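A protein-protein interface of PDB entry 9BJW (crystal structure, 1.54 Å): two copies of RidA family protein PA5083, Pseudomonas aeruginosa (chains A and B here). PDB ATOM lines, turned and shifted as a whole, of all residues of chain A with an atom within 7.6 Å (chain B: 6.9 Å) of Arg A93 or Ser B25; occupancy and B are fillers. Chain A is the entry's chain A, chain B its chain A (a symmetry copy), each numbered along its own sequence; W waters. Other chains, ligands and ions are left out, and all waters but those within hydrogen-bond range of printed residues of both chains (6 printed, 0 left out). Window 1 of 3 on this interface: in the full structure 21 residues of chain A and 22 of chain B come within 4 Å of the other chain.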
ATOM      1  N   LEU A  61       2.680   0.961  -1.697  1.00  0.00           N
ATOM      2  CA  LEU A  61       2.468   2.399  -1.718  1.00  0.00           C
ATOM      3  C   LEU A  61       3.077   3.092  -0.510  1.00  0.00           C
ATOM      4  O   LEU A  61       3.712   4.145  -0.657  1.00  0.00           O
ATOM      5  CB  LEU A  61       0.965   2.701  -1.788  1.00  0.00           C
ATOM      6  CG  LEU A  61       0.265   2.093  -3.007  1.00  0.00           C
ATOM      7  CD1 LEU A  61      -1.231   2.348  -2.947  1.00  0.00           C
ATOM      8  CD2 LEU A  61       0.853   2.634  -4.306  1.00  0.00           C
ATOM      9  N   SER A  62       2.922   2.498   0.670  1.00  0.00           N
ATOM     10  CA  SER A  62       3.441   3.085   1.896  1.00  0.00           C
ATOM     11  C   SER A  62       3.812   1.985   2.877  1.00  0.00           C
ATOM     12  O   SER A  62       3.180   0.924   2.928  1.00  0.00           O
ATOM     13  CB  SER A  62       2.408   4.018   2.539  1.00  0.00           C
ATOM     14  OG  SER A  62       1.271   3.279   2.960  1.00  0.00           O
ATOM     15  N   ALA A  63       4.820   2.274   3.692  1.00  0.00           N
ATOM     16  CA  ALA A  63       5.219   1.412   4.789  1.00  0.00           C
ATOM     17  C   ALA A  63       5.510   2.297   5.985  1.00  0.00           C
ATOM     18  O   ALA A  63       6.294   3.240   5.871  1.00  0.00           O
ATOM     19  CB  ALA A  63       6.470   0.588   4.437  1.00  0.00           C
ATOM     20  N   THR A  64       4.870   2.014   7.114  1.00  0.00           N
ATOM     21  CA  THR A  64       5.288   2.574   8.394  1.00  0.00           C
ATOM     22  C   THR A  64       6.043   1.482   9.138  1.00  0.00           C
ATOM     23  O   THR A  64       5.519   0.378   9.343  1.00  0.00           O
ATOM     24  CB  THR A  64       4.112   3.102   9.220  1.00  0.00           C
ATOM     25  OG1 THR A  64       3.480   4.173   8.499  1.00  0.00           O
ATOM     26  CG2 THR A  64       4.615   3.659  10.547  1.00  0.00           C
ATOM     27  N   ILE A  65       7.278   1.788   9.517  1.00  0.00           N
ATOM     28  CA  ILE A  65       8.171   0.851  10.188  1.00  0.00           C
ATOM     29  C   ILE A  65       8.311   1.308  11.631  1.00  0.00           C
ATOM     30  O   ILE A  65       8.708   2.453  11.886  1.00  0.00           O
ATOM     31  CB  ILE A  65       9.545   0.792   9.496  1.00  0.00           C
ATOM     32  CG1 ILE A  65       9.372   0.385   8.021  1.00  0.00           C
ATOM     33  CG2 ILE A  65      10.502  -0.133  10.252  1.00  0.00           C
ATOM     34  CD1 ILE A  65      10.660   0.409   7.199  1.00  0.00           C
ATOM     35  N   LEU A  67      10.170   0.611  15.211  1.00  0.00           N
ATOM     36  CA  LEU A  67      11.306  -0.025  15.867  1.00  0.00           C
ATOM     37  C   LEU A  67      11.217   0.179  17.373  1.00  0.00           C
ATOM     38  O   LEU A  67      10.976   1.298  17.838  1.00  0.00           O
ATOM     39  CB  LEU A  67      12.625   0.543  15.324  1.00  0.00           C
ATOM     40  CG  LEU A  67      12.954   0.177  13.877  1.00  0.00           C
ATOM     41  CD1 LEU A  67      14.106   1.017  13.360  1.00  0.00           C
ATOM     42  CD2 LEU A  67      13.283  -1.308  13.781  1.00  0.00           C
ATOM     43  N   PHE A  74      18.188   1.037  13.659  1.00  0.00           N
ATOM     44  CA  PHE A  74      17.859   1.682  12.389  1.00  0.00           C
ATOM     45  C   PHE A  74      18.780   1.208  11.269  1.00  0.00           C
ATOM     46  O   PHE A  74      18.318   0.920  10.160  1.00  0.00           O
ATOM     47  CB  PHE A  74      17.928   3.205  12.555  1.00  0.00           C
ATOM     48  CG  PHE A  74      17.403   3.996  11.380  1.00  0.00           C
ATOM     49  CD1 PHE A  74      16.118   3.798  10.894  1.00  0.00           C
ATOM     50  CD2 PHE A  74      18.184   4.982  10.800  1.00  0.00           C
ATOM     51  CE1 PHE A  74      15.641   4.542   9.829  1.00  0.00           C
ATOM     52  CE2 PHE A  74      17.716   5.734   9.754  1.00  0.00           C
ATOM     53  CZ  PHE A  74      16.435   5.514   9.256  1.00  0.00           C
ATOM     54  N   LEU A  77      17.907  -2.415  10.314  1.00  0.00           N
ATOM     55  CA  LEU A  77      16.641  -2.364   9.589  1.00  0.00           C
ATOM     56  C   LEU A  77      16.867  -1.933   8.147  1.00  0.00           C
ATOM     57  O   LEU A  77      16.351  -2.554   7.204  1.00  0.00           O
ATOM     58  CB  LEU A  77      15.685  -1.405  10.314  1.00  0.00           C
ATOM     59  CG  LEU A  77      14.297  -1.065   9.733  1.00  0.00           C
ATOM     60  CD1 LEU A  77      14.344  -0.012   8.623  1.00  0.00           C
ATOM     61  CD2 LEU A  77      13.564  -2.328   9.271  1.00  0.00           C
ATOM     62  N   ASN A  78      17.633  -0.863   7.951  1.00  0.00           N
ATOM     63  CA  ASN A  78      17.847  -0.351   6.603  1.00  0.00           C
ATOM     64  C   ASN A  78      18.601  -1.358   5.739  1.00  0.00           C
ATOM     65  O   ASN A  78      18.310  -1.499   4.548  1.00  0.00           O
ATOM     66  CB  ASN A  78      18.591   0.983   6.653  1.00  0.00           C
ATOM     67  CG  ASN A  78      17.696   2.144   7.043  1.00  0.00           C
ATOM     68  OD1 ASN A  78      16.514   2.176   6.708  1.00  0.00           O
ATOM     69  ND2 ASN A  78      18.262   3.109   7.761  1.00  0.00           N
ATOM     70  N   GLU A  79      19.563  -2.075   6.321  1.00  0.00           N
ATOM     71  CA  GLU A  79      20.322  -3.058   5.552  1.00  0.00           C
ATOM     72  C   GLU A  79      19.406  -4.132   4.970  1.00  0.00           C
ATOM     73  O   GLU A  79      19.450  -4.420   3.766  1.00  0.00           O
ATOM     74  CB  GLU A  79      21.409  -3.673   6.442  1.00  0.00           C
ATOM     75  CG  GLU A  79      22.290  -4.717   5.778  1.00  0.00           C
ATOM     76  CD  GLU A  79      23.284  -5.335   6.755  1.00  0.00           C
ATOM     77  OE1 GLU A  79      23.550  -4.721   7.815  1.00  0.00           O
ATOM     78  OE2 GLU A  79      23.794  -6.438   6.471  1.00  0.00           O
ATOM     79  N   TRP A  81      16.023  -4.099   4.795  1.00  0.00           N
ATOM     80  CA  TRP A  81      14.983  -3.458   4.000  1.00  0.00           C
ATOM     81  C   TRP A  81      15.461  -3.157   2.581  1.00  0.00           C
ATOM     82  O   TRP A  81      14.781  -3.488   1.603  1.00  0.00           O
ATOM     83  CB  TRP A  81      14.546  -2.184   4.729  1.00  0.00           C
ATOM     84  CG  TRP A  81      13.652  -1.278   3.973  1.00  0.00           C
ATOM     85  CD1 TRP A  81      14.015  -0.146   3.314  1.00  0.00           C
ATOM     86  CD2 TRP A  81      12.234  -1.397   3.816  1.00  0.00           C
ATOM     87  NE1 TRP A  81      12.918   0.453   2.758  1.00  0.00           N
ATOM     88  CE2 TRP A  81      11.811  -0.300   3.047  1.00  0.00           C
ATOM     89  CE3 TRP A  81      11.286  -2.324   4.253  1.00  0.00           C
ATOM     90  CZ2 TRP A  81      10.476  -0.103   2.698  1.00  0.00           C
ATOM     91  CZ3 TRP A  81       9.953  -2.132   3.898  1.00  0.00           C
ATOM     92  CH2 TRP A  81       9.565  -1.027   3.137  1.00  0.00           C
ATOM     93  N   THR A  82      16.636  -2.536   2.441  1.00  0.00           N
ATOM     94  CA  THR A  82      17.083  -2.146   1.105  1.00  0.00           C
ATOM     95  C   THR A  82      17.384  -3.359   0.232  1.00  0.00           C
ATOM     96  O   THR A  82      17.180  -3.309  -0.986  1.00  0.00           O
ATOM     97  CB  THR A  82      18.316  -1.244   1.188  1.00  0.00           C
ATOM     98  OG1 THR A  82      19.321  -1.880   1.982  1.00  0.00           O
ATOM     99  CG2 THR A  82      17.957   0.094   1.808  1.00  0.00           C
ATOM    100  N   LEU A  85      13.909  -4.885  -1.033  1.00  0.00           N
ATOM    101  CA  LEU A  85      13.102  -4.106  -1.959  1.00  0.00           C
ATOM    102  C   LEU A  85      13.479  -4.404  -3.410  1.00  0.00           C
ATOM    103  O   LEU A  85      14.650  -4.648  -3.720  1.00  0.00           O
ATOM    104  CB  LEU A  85      13.276  -2.615  -1.705  1.00  0.00           C
ATOM    105  CG  LEU A  85      12.558  -1.972  -0.513  1.00  0.00           C
ATOM    106  CD1 LEU A  85      12.891  -0.500  -0.481  1.00  0.00           C
ATOM    107  CD2 LEU A  85      11.049  -2.193  -0.588  1.00  0.00           C
ATOM    108  N   ALA A  90      11.350   1.674  -4.538  1.00  0.00           N
ATOM    109  CA  ALA A  90      11.040   1.778  -3.120  1.00  0.00           C
ATOM    110  C   ALA A  90       9.741   2.551  -2.895  1.00  0.00           C
ATOM    111  O   ALA A  90       9.423   3.488  -3.634  1.00  0.00           O
ATOM    112  CB  ALA A  90      12.180   2.452  -2.363  1.00  0.00           C
ATOM    113  N   PRO A  91       8.981   2.180  -1.853  1.00  0.00           N
ATOM    114  CA  PRO A  91       7.709   2.854  -1.560  1.00  0.00           C
ATOM    115  C   PRO A  91       7.899   4.100  -0.703  1.00  0.00           C
ATOM    116  O   PRO A  91       9.021   4.385  -0.271  1.00  0.00           O
ATOM    117  CB  PRO A  91       6.942   1.776  -0.787  1.00  0.00           C
ATOM    118  CG  PRO A  91       8.051   1.120   0.035  1.00  0.00           C
ATOM    119  CD  PRO A  91       9.249   1.082  -0.906  1.00  0.00           C
ATOM    120  N   SER A  92       6.824   4.846  -0.437  1.00  0.00           N
ATOM    121  CA  SER A  92       6.906   5.858   0.610  1.00  0.00           C
ATOM    122  C   SER A  92       7.083   5.167   1.952  1.00  0.00           C
ATOM    123  O   SER A  92       6.608   4.049   2.166  1.00  0.00           O
ATOM    124  CB  SER A  92       5.660   6.755   0.618  1.00  0.00           C
ATOM    125  OG  SER A  92       4.498   6.098   1.117  1.00  0.00           O
ATOM    126  N   ARG A  93       7.821   5.809   2.855  1.00  0.00           N
ATOM    127  CA  ARG A  93       8.010   5.146   4.131  1.00  0.00           C
ATOM    128  C   ARG A  93       8.260   6.136   5.260  1.00  0.00           C
ATOM    129  O   ARG A  93       8.713   7.270   5.060  1.00  0.00           O
ATOM    130  CB  ARG A  93       9.114   4.083   4.048  1.00  0.00           C
ATOM    131  CG  ARG A  93      10.482   4.526   4.267  1.00  0.00           C
ATOM    132  CD  ARG A  93      11.386   3.351   4.682  1.00  0.00           C
ATOM    133  NE  ARG A  93      12.494   3.953   5.396  1.00  0.00           N
ATOM    134  CZ  ARG A  93      13.610   3.350   5.779  1.00  0.00           C
ATOM    135  NH1 ARG A  93      13.846   2.077   5.508  1.00  0.00           N
ATOM    136  NH2 ARG A  93      14.510   4.048   6.465  1.00  0.00           N
ATOM    137  N   THR A  94       7.921   5.675   6.456  1.00  0.00           N
ATOM    138  CA  THR A  94       8.082   6.408   7.701  1.00  0.00           C
ATOM    139  C   THR A  94       8.618   5.422   8.724  1.00  0.00           C
ATOM    140  O   THR A  94       8.069   4.329   8.866  1.00  0.00           O
ATOM    141  CB  THR A  94       6.739   6.983   8.174  1.00  0.00           C
ATOM    142  OG1 THR A  94       6.201   7.853   7.166  1.00  0.00           O
ATOM    143  CG2 THR A  94       6.897   7.723   9.487  1.00  0.00           C
ATOM    144  N   THR A  95       9.687   5.789   9.428  1.00  0.00           N
ATOM    145  CA  THR A  95      10.298   4.921  10.425  1.00  0.00           C
ATOM    146  C   THR A  95      10.340   5.673  11.751  1.00  0.00           C
ATOM    147  O   THR A  95      10.935   6.754  11.838  1.00  0.00           O
ATOM    148  CB  THR A  95      11.704   4.477  10.004  1.00  0.00           C
ATOM    149  OG1 THR A  95      11.637   3.903   8.688  1.00  0.00           O
ATOM    150  CG2 THR A  95      12.223   3.448  10.958  1.00  0.00           C
ATOM    151  N   ALA B   7      11.458  11.085  -6.388  1.00  0.00           N
ATOM    152  CA  ALA B   7      12.640  11.156  -5.522  1.00  0.00           C
ATOM    153  C   ALA B   7      12.870   9.826  -4.801  1.00  0.00           C
ATOM    154  O   ALA B   7      12.718   9.690  -3.580  1.00  0.00           O
ATOM    155  CB  ALA B   7      12.528  12.320  -4.531  1.00  0.00           C
ATOM    156  N   ASP B  10      17.495   4.214  -2.274  1.00  0.00           N
ATOM    157  CA  ASP B  10      17.512   2.791  -1.958  1.00  0.00           C
ATOM    158  C   ASP B  10      16.535   2.415  -0.851  1.00  0.00           C
ATOM    159  O   ASP B  10      16.169   1.241  -0.744  1.00  0.00           O
ATOM    160  CB  ASP B  10      18.926   2.362  -1.567  1.00  0.00           C
ATOM    161  CG  ASP B  10      19.880   2.387  -2.739  1.00  0.00           C
ATOM    162  OD1 ASP B  10      19.448   2.014  -3.851  1.00  0.00           O
ATOM    163  OD2 ASP B  10      21.046   2.793  -2.551  1.00  0.00           O
ATOM    164  N   ARG B  11      16.106   3.376  -0.031  1.00  0.00           N
ATOM    165  CA  ARG B  11      15.218   3.089   1.090  1.00  0.00           C
ATOM    166  C   ARG B  11      13.769   3.481   0.841  1.00  0.00           C
ATOM    167  O   ARG B  11      12.862   2.822   1.364  1.00  0.00           O
ATOM    168  CB  ARG B  11      15.682   3.821   2.351  1.00  0.00           C
ATOM    169  CG  ARG B  11      17.102   3.551   2.765  1.00  0.00           C
ATOM    170  CD  ARG B  11      17.467   4.484   3.902  1.00  0.00           C
ATOM    171  NE  ARG B  11      18.811   4.239   4.407  1.00  0.00           N
ATOM    172  CZ  ARG B  11      19.396   4.965   5.350  1.00  0.00           C
ATOM    173  NH1 ARG B  11      18.775   5.987   5.919  1.00  0.00           N
ATOM    174  NH2 ARG B  11      20.634   4.660   5.729  1.00  0.00           N
ATOM    175  N   LEU B  12      13.530   4.568   0.114  1.00  0.00           N
ATOM    176  CA  LEU B  12      12.185   5.120   0.024  1.00  0.00           C
ATOM    177  C   LEU B  12      12.060   6.008  -1.206  1.00  0.00           C
ATOM    178  O   LEU B  12      13.053   6.447  -1.795  1.00  0.00           O
ATOM    179  CB  LEU B  12      11.831   5.907   1.289  1.00  0.00           C
ATOM    180  CG  LEU B  12      12.754   7.059   1.701  1.00  0.00           C
ATOM    181  CD1 LEU B  12      12.431   8.354   0.959  1.00  0.00           C
ATOM    182  CD2 LEU B  12      12.651   7.280   3.205  1.00  0.00           C
ATOM    183  N   SER B  13      10.812   6.300  -1.562  1.00  0.00           N
ATOM    184  CA  SER B  13      10.485   7.371  -2.491  1.00  0.00           C
ATOM    185  C   SER B  13       9.788   8.472  -1.703  1.00  0.00           C
ATOM    186  O   SER B  13       8.907   8.188  -0.878  1.00  0.00           O
ATOM    187  CB  SER B  13       9.585   6.889  -3.641  1.00  0.00           C
ATOM    188  OG  SER B  13      10.226   5.910  -4.442  1.00  0.00           O
ATOM    189  N   ALA B  14      10.198   9.719  -1.940  1.00  0.00           N
ATOM    190  CA  ALA B  14       9.584  10.842  -1.240  1.00  0.00           C
ATOM    191  C   ALA B  14       8.076  10.863  -1.445  1.00  0.00           C
ATOM    192  O   ALA B  14       7.322  11.195  -0.523  1.00  0.00           O
ATOM    193  CB  ALA B  14      10.212  12.158  -1.701  1.00  0.00           C
ATOM    194  N   ALA B  15       7.611  10.525  -2.648  1.00  0.00           N
ATOM    195  CA  ALA B  15       6.183  10.423  -2.899  1.00  0.00           C
ATOM    196  C   ALA B  15       5.913   9.223  -3.793  1.00  0.00           C
ATOM    197  O   ALA B  15       6.711   8.903  -4.677  1.00  0.00           O
ATOM    198  CB  ALA B  15       5.626  11.692  -3.553  1.00  0.00           C
ATOM    199  N   VAL B  16       4.801   8.546  -3.538  1.00  0.00           N
ATOM    200  CA  VAL B  16       4.290   7.511  -4.427  1.00  0.00           C
ATOM    201  C   VAL B  16       2.857   7.865  -4.781  1.00  0.00           C
ATOM    202  O   VAL B  16       2.036   8.125  -3.894  1.00  0.00           O
ATOM    203  CB  VAL B  16       4.372   6.107  -3.805  1.00  0.00           C
ATOM    204  CG1 VAL B  16       3.698   5.087  -4.717  1.00  0.00           C
ATOM    205  CG2 VAL B  16       5.816   5.720  -3.559  1.00  0.00           C
ATOM    206  N   PHE B  23       0.902   9.340  -1.649  1.00  0.00           N
ATOM    207  CA  PHE B  23       1.450   8.900  -0.364  1.00  0.00           C
ATOM    208  C   PHE B  23       2.838   9.506  -0.183  1.00  0.00           C
ATOM    209  O   PHE B  23       3.758   9.195  -0.944  1.00  0.00           O
ATOM    210  CB  PHE B  23       1.537   7.369  -0.295  1.00  0.00           C
ATOM    211  CG  PHE B  23       0.209   6.667  -0.418  1.00  0.00           C
ATOM    212  CD1 PHE B  23      -0.385   6.499  -1.663  1.00  0.00           C
ATOM    213  CD2 PHE B  23      -0.427   6.150   0.705  1.00  0.00           C
ATOM    214  CE1 PHE B  23      -1.612   5.850  -1.787  1.00  0.00           C
ATOM    215  CE2 PHE B  23      -1.654   5.491   0.584  1.00  0.00           C
ATOM    216  CZ  PHE B  23      -2.239   5.343  -0.668  1.00  0.00           C
ATOM    217  N   LEU B  24       3.010  10.330   0.846  1.00  0.00           N
ATOM    218  CA  LEU B  24       4.312  10.940   1.091  1.00  0.00           C
ATOM    219  C   LEU B  24       5.067  10.182   2.172  1.00  0.00           C
ATOM    220  O   LEU B  24       4.474   9.736   3.157  1.00  0.00           O
ATOM    221  CB  LEU B  24       4.165  12.403   1.506  1.00  0.00           C
ATOM    222  CG  LEU B  24       3.453  13.336   0.527  1.00  0.00           C
ATOM    223  CD1 LEU B  24       3.611  14.767   1.013  1.00  0.00           C
ATOM    224  CD2 LEU B  24       3.974  13.183  -0.895  1.00  0.00           C
ATOM    225  N   SER B  25       6.376  10.037   1.981  1.00  0.00           N
ATOM    226  CA  SER B  25       7.233   9.603   3.072  1.00  0.00           C
ATOM    227  C   SER B  25       7.164  10.604   4.224  1.00  0.00           C
ATOM    228  O   SER B  25       6.923  11.799   4.028  1.00  0.00           O
ATOM    229  CB  SER B  25       8.679   9.457   2.594  1.00  0.00           C
ATOM    230  OG  SER B  25       8.850   8.307   1.779  1.00  0.00           O
ATOM    231  N   GLY B  26       7.352  10.100   5.439  1.00  0.00           N
ATOM    232  CA  GLY B  26       7.506  10.989   6.577  1.00  0.00           C
ATOM    233  C   GLY B  26       8.564  12.037   6.288  1.00  0.00           C
ATOM    234  O   GLY B  26       9.673  11.694   5.868  1.00  0.00           O
ATOM    235  N   GLN B  27       8.227  13.305   6.481  1.00  0.00           N
ATOM    236  CA  GLN B  27       9.146  14.407   6.220  1.00  0.00           C
ATOM    237  C   GLN B  27       9.762  14.876   7.527  1.00  0.00           C
ATOM    238  O   GLN B  27       9.069  15.010   8.543  1.00  0.00           O
ATOM    239  CB  GLN B  27       8.436  15.562   5.501  1.00  0.00           C
ATOM    240  CG  GLN B  27       8.024  15.220   4.055  1.00  0.00           C
ATOM    241  CD  GLN B  27       9.201  14.696   3.261  1.00  0.00           C
ATOM    242  OE1 GLN B  27      10.193  15.400   3.057  1.00  0.00           O
ATOM    243  NE2 GLN B  27       9.112  13.446   2.828  1.00  0.00           N
ATOM    244  N   VAL B  28      11.067  15.115   7.492  1.00  0.00           N
ATOM    245  CA  VAL B  28      11.832  15.504   8.669  1.00  0.00           C
ATOM    246  C   VAL B  28      12.335  16.923   8.446  1.00  0.00           C
ATOM    247  O   VAL B  28      12.299  17.431   7.312  1.00  0.00           O
ATOM    248  CB  VAL B  28      12.985  14.514   8.955  1.00  0.00           C
ATOM    249  CG1 VAL B  28      12.422  13.146   9.353  1.00  0.00           C
ATOM    250  CG2 VAL B  28      13.898  14.396   7.758  1.00  0.00           C
ATOM    251  N   ILE B  46       6.708  19.163   2.823  1.00  0.00           N
ATOM    252  CA  ILE B  46       5.463  18.516   2.421  1.00  0.00           C
ATOM    253  C   ILE B  46       4.795  19.305   1.300  1.00  0.00           C
ATOM    254  O   ILE B  46       4.318  18.730   0.316  1.00  0.00           O
ATOM    255  CB  ILE B  46       4.549  18.346   3.652  1.00  0.00           C
ATOM    256  CG1 ILE B  46       5.105  17.252   4.561  1.00  0.00           C
ATOM    257  CG2 ILE B  46       3.102  18.037   3.244  1.00  0.00           C
ATOM    258  CD1 ILE B  46       4.338  17.104   5.856  1.00  0.00           C
ATOM    259  N   LEU B  49       6.436  18.619  -2.035  1.00  0.00           N
ATOM    260  CA  LEU B  49       6.130  17.283  -2.535  1.00  0.00           C
ATOM    261  C   LEU B  49       4.698  17.198  -3.049  1.00  0.00           C
ATOM    262  O   LEU B  49       4.448  16.571  -4.084  1.00  0.00           O
ATOM    263  CB  LEU B  49       6.379  16.242  -1.440  1.00  0.00           C
ATOM    264  CG  LEU B  49       7.850  15.921  -1.184  1.00  0.00           C
ATOM    265  CD1 LEU B  49       7.979  15.059   0.053  1.00  0.00           C
ATOM    266  CD2 LEU B  49       8.490  15.231  -2.389  1.00  0.00           C
ATOM    267  N   GLU B 108       8.154  14.929  12.914  1.00  0.00           N
ATOM    268  CA  GLU B 108       8.107  14.277  11.612  1.00  0.00           C
ATOM    269  C   GLU B 108       6.639  14.108  11.248  1.00  0.00           C
ATOM    270  O   GLU B 108       5.823  13.788  12.116  1.00  0.00           O
ATOM    271  CB  GLU B 108       8.831  12.929  11.633  1.00  0.00           C
ATOM    272  CG  GLU B 108       8.674  12.148  10.323  1.00  0.00           C
ATOM    273  CD  GLU B 108       9.617  10.976  10.199  1.00  0.00           C
ATOM    274  OE1 GLU B 108      10.519  10.810  11.048  1.00  0.00           O
ATOM    275  OE2 GLU B 108       9.450  10.201   9.217  1.00  0.00           O
ATOM    276  N   ILE B 109       6.280  14.353   9.985  1.00  0.00           N
ATOM    277  CA  ILE B 109       4.872  14.330   9.600  1.00  0.00           C
ATOM    278  C   ILE B 109       4.696  13.525   8.318  1.00  0.00           C
ATOM    279  O   ILE B 109       5.410  13.751   7.331  1.00  0.00           O
ATOM    280  CB  ILE B 109       4.297  15.753   9.429  1.00  0.00           C
ATOM    281  CG1 ILE B 109       4.463  16.559  10.730  1.00  0.00           C
ATOM    282  CG2 ILE B 109       2.839  15.709   8.968  1.00  0.00           C
ATOM    283  CD1 ILE B 109       3.939  17.993  10.623  1.00  0.00           C
ATOM    284  N   THR B 110       3.748  12.585   8.337  1.00  0.00           N
ATOM    285  CA  THR B 110       3.442  11.714   7.203  1.00  0.00           C
ATOM    286  C   THR B 110       2.066  12.055   6.637  1.00  0.00           C
ATOM    287  O   THR B 110       1.063  11.988   7.354  1.00  0.00           O
ATOM    288  CB  THR B 110       3.485  10.253   7.643  1.00  0.00           C
ATOM    289  OG1 THR B 110       4.779   9.965   8.183  1.00  0.00           O
ATOM    290  CG2 THR B 110       3.179   9.320   6.471  1.00  0.00           C
ATOM    291  N   VAL B 111       2.007  12.373   5.343  1.00  0.00           N
ATOM    292  CA  VAL B 111       0.792  12.870   4.704  1.00  0.00           C
ATOM    293  C   VAL B 111       0.329  11.936   3.581  1.00  0.00           C
ATOM    294  O   VAL B 111       1.141  11.401   2.818  1.00  0.00           O
ATOM    295  CB  VAL B 111       1.015  14.303   4.161  1.00  0.00           C
ATOM    296  CG1 VAL B 111       0.064  14.641   3.014  1.00  0.00           C
ATOM    297  CG2 VAL B 111       0.865  15.330   5.299  1.00  0.00           C
HETATM  298  O   HOH W   1      10.705   9.078   6.068  1.00  0.00           O
HETATM  299  O   HOH W   2      21.212   3.396   8.157  1.00  0.00           O
HETATM  300  O   HOH W   3       3.269   7.337   3.335  1.00  0.00           O
HETATM  301  O   HOH W   4      16.528  -0.951  -2.295  1.00  0.00           O
HETATM  302  O   HOH W   5      10.990   8.283   8.611  1.00  0.00           O
HETATM  303  O   HOH W   6      12.497   8.878  11.712  1.00  0.00           O
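The side-chain amide nitrogen of Asn A78 sits close to the guanidinium group of Arg B11, at 3.5 Å.
The indole nitrogen of Trp A81 sits at hydrogen-bond distance from the backbone carbonyl oxygen of Arg B11, 2.7 Å away.
The backbone carbonyl oxygen (O) of Ala A90 is in hydrogen-bond range of the side-chain hydroxyl (OG) of Ser B13 (2.7 Å).
The backbone NH (N) of Ser B13 sits at hydrogen-bond distance from the backbone carbonyl oxygen (O) of Pro A91.
N of Arg A93 sits at hydrogen-bond distance from OG of Ser B25 (2.9 Å).
The backbone NH (N) of Gly B26 sits at hydrogen-bond distance from the backbone carbonyl oxygen (O) of Arg A93, at 3.2 Å.
The side-chain hydroxyl of Thr A94 lies within hydrogen-bond range of the backbone NH of Gly B26 (3.1 Å).
The side-chain hydroxyl (OG1) of Thr A94 is in hydrogen-bond range of the side-chain hydroxyl (OG1) of Thr B110 (2.7 Å).
The backbone NH (N) of Ala A63 lies within hydrogen-bond range of the backbone carbonyl oxygen (O) of Ser A92.
The backbone carbonyl oxygen of Thr A94 is in hydrogen-bond range of the backbone NH of Ile A65.
The guanidinium group (NE) of Arg A93 lies within hydrogen-bond range of the side-chain hydroxyl (OG1) of Thr A95 (3.4 Å).
N of Leu B24 lies within hydrogen-bond range of O of Val B111 (2.9 Å).
O of Asp B10 touches CG2 of Thr A82, 3.3 Å away.
CG2 of Thr A82 touches CG of Arg B11, at 3.7 Å.
O of Asp B10 touches CD1 of Leu A85, at 3.7 Å.
Ala A90 touches Arg B11 (CB to C, 3.7 Å).
Ala A90 touches Leu B12.
Val B16 touches Ser A92.
Ser A92 touches Phe B23 (CB to O, 3.5 Å).
Ser A92 touches Leu B24.
Arg A93 touches Leu B12 (CG to CB, 3.5 Å).
Thr A94 touches Glu B108.
Of the printed residues of chain B, Ser A62 touches Phe B23.
Of chain B, only Arg B11, Leu B12, Ser B25 and Gly B26 come within 4 Å of Arg A93.
Printed residues of chain B within 4 Å of Thr A94: Gly B26, Glu B108 and Thr B110.
Of the printed residues of chain A, Phe B23 touches Leu A61 (3.7 Å), Ser A62 (3.99 Å) and Ser A92 (3.5 Å).
Of the printed residues of chain A, Leu B24 touches Ser A92 (3.8 Å).
Of chain A, only Ser A92 and Arg A93 come within 4 Å of Ser B25.
Of chain A, only Arg A93 and Thr A94 come within 4 Å of Gly B26.
Printed residues of chain A within 4 Å of Thr B110: Thr A94 (2.7 Å).
The nearest printed residue of chain B that does not touch Ser A62 is Val B16 (5.9 Å).
Of the 20 printed residues of chain B, 11 touch a printed residue of chain A.
Hydrophobic or aromatic side chains of chain B within 4 Å of the printed part of chain A: Leu B12, Val B16 and Phe B23.
Along chain B the printed residues that touch a printed residue of chain A span positions 10 to 110.
Of the 19 printed residues of chain A, 12 touch a printed residue of chain B.
Hydrophobic or aromatic side chains of chain A that line the printed part of chain B: Leu A61, Phe A74, Trp A81, Leu A85 and Ala A90.
Among the printed residues, 28 pairs touch across the chains.
No position is printed for both chains.
Of the 28 pairs that touch across the chains among the printed residues, none has its exchanged pair printed and touching as well.
Water W2 lies within hydrogen-bond range of the guanidinium group (NH2) of Arg B11 (2.8 Å) and the side-chain amide nitrogen (ND2) of Asn A78 (3.0 Å).
Water W1 bridges the backbone carbonyl oxygen (O) of Gly B26 (2.8 Å) and the backbone carbonyl oxygen (O) of Arg A93 (2.9 Å).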
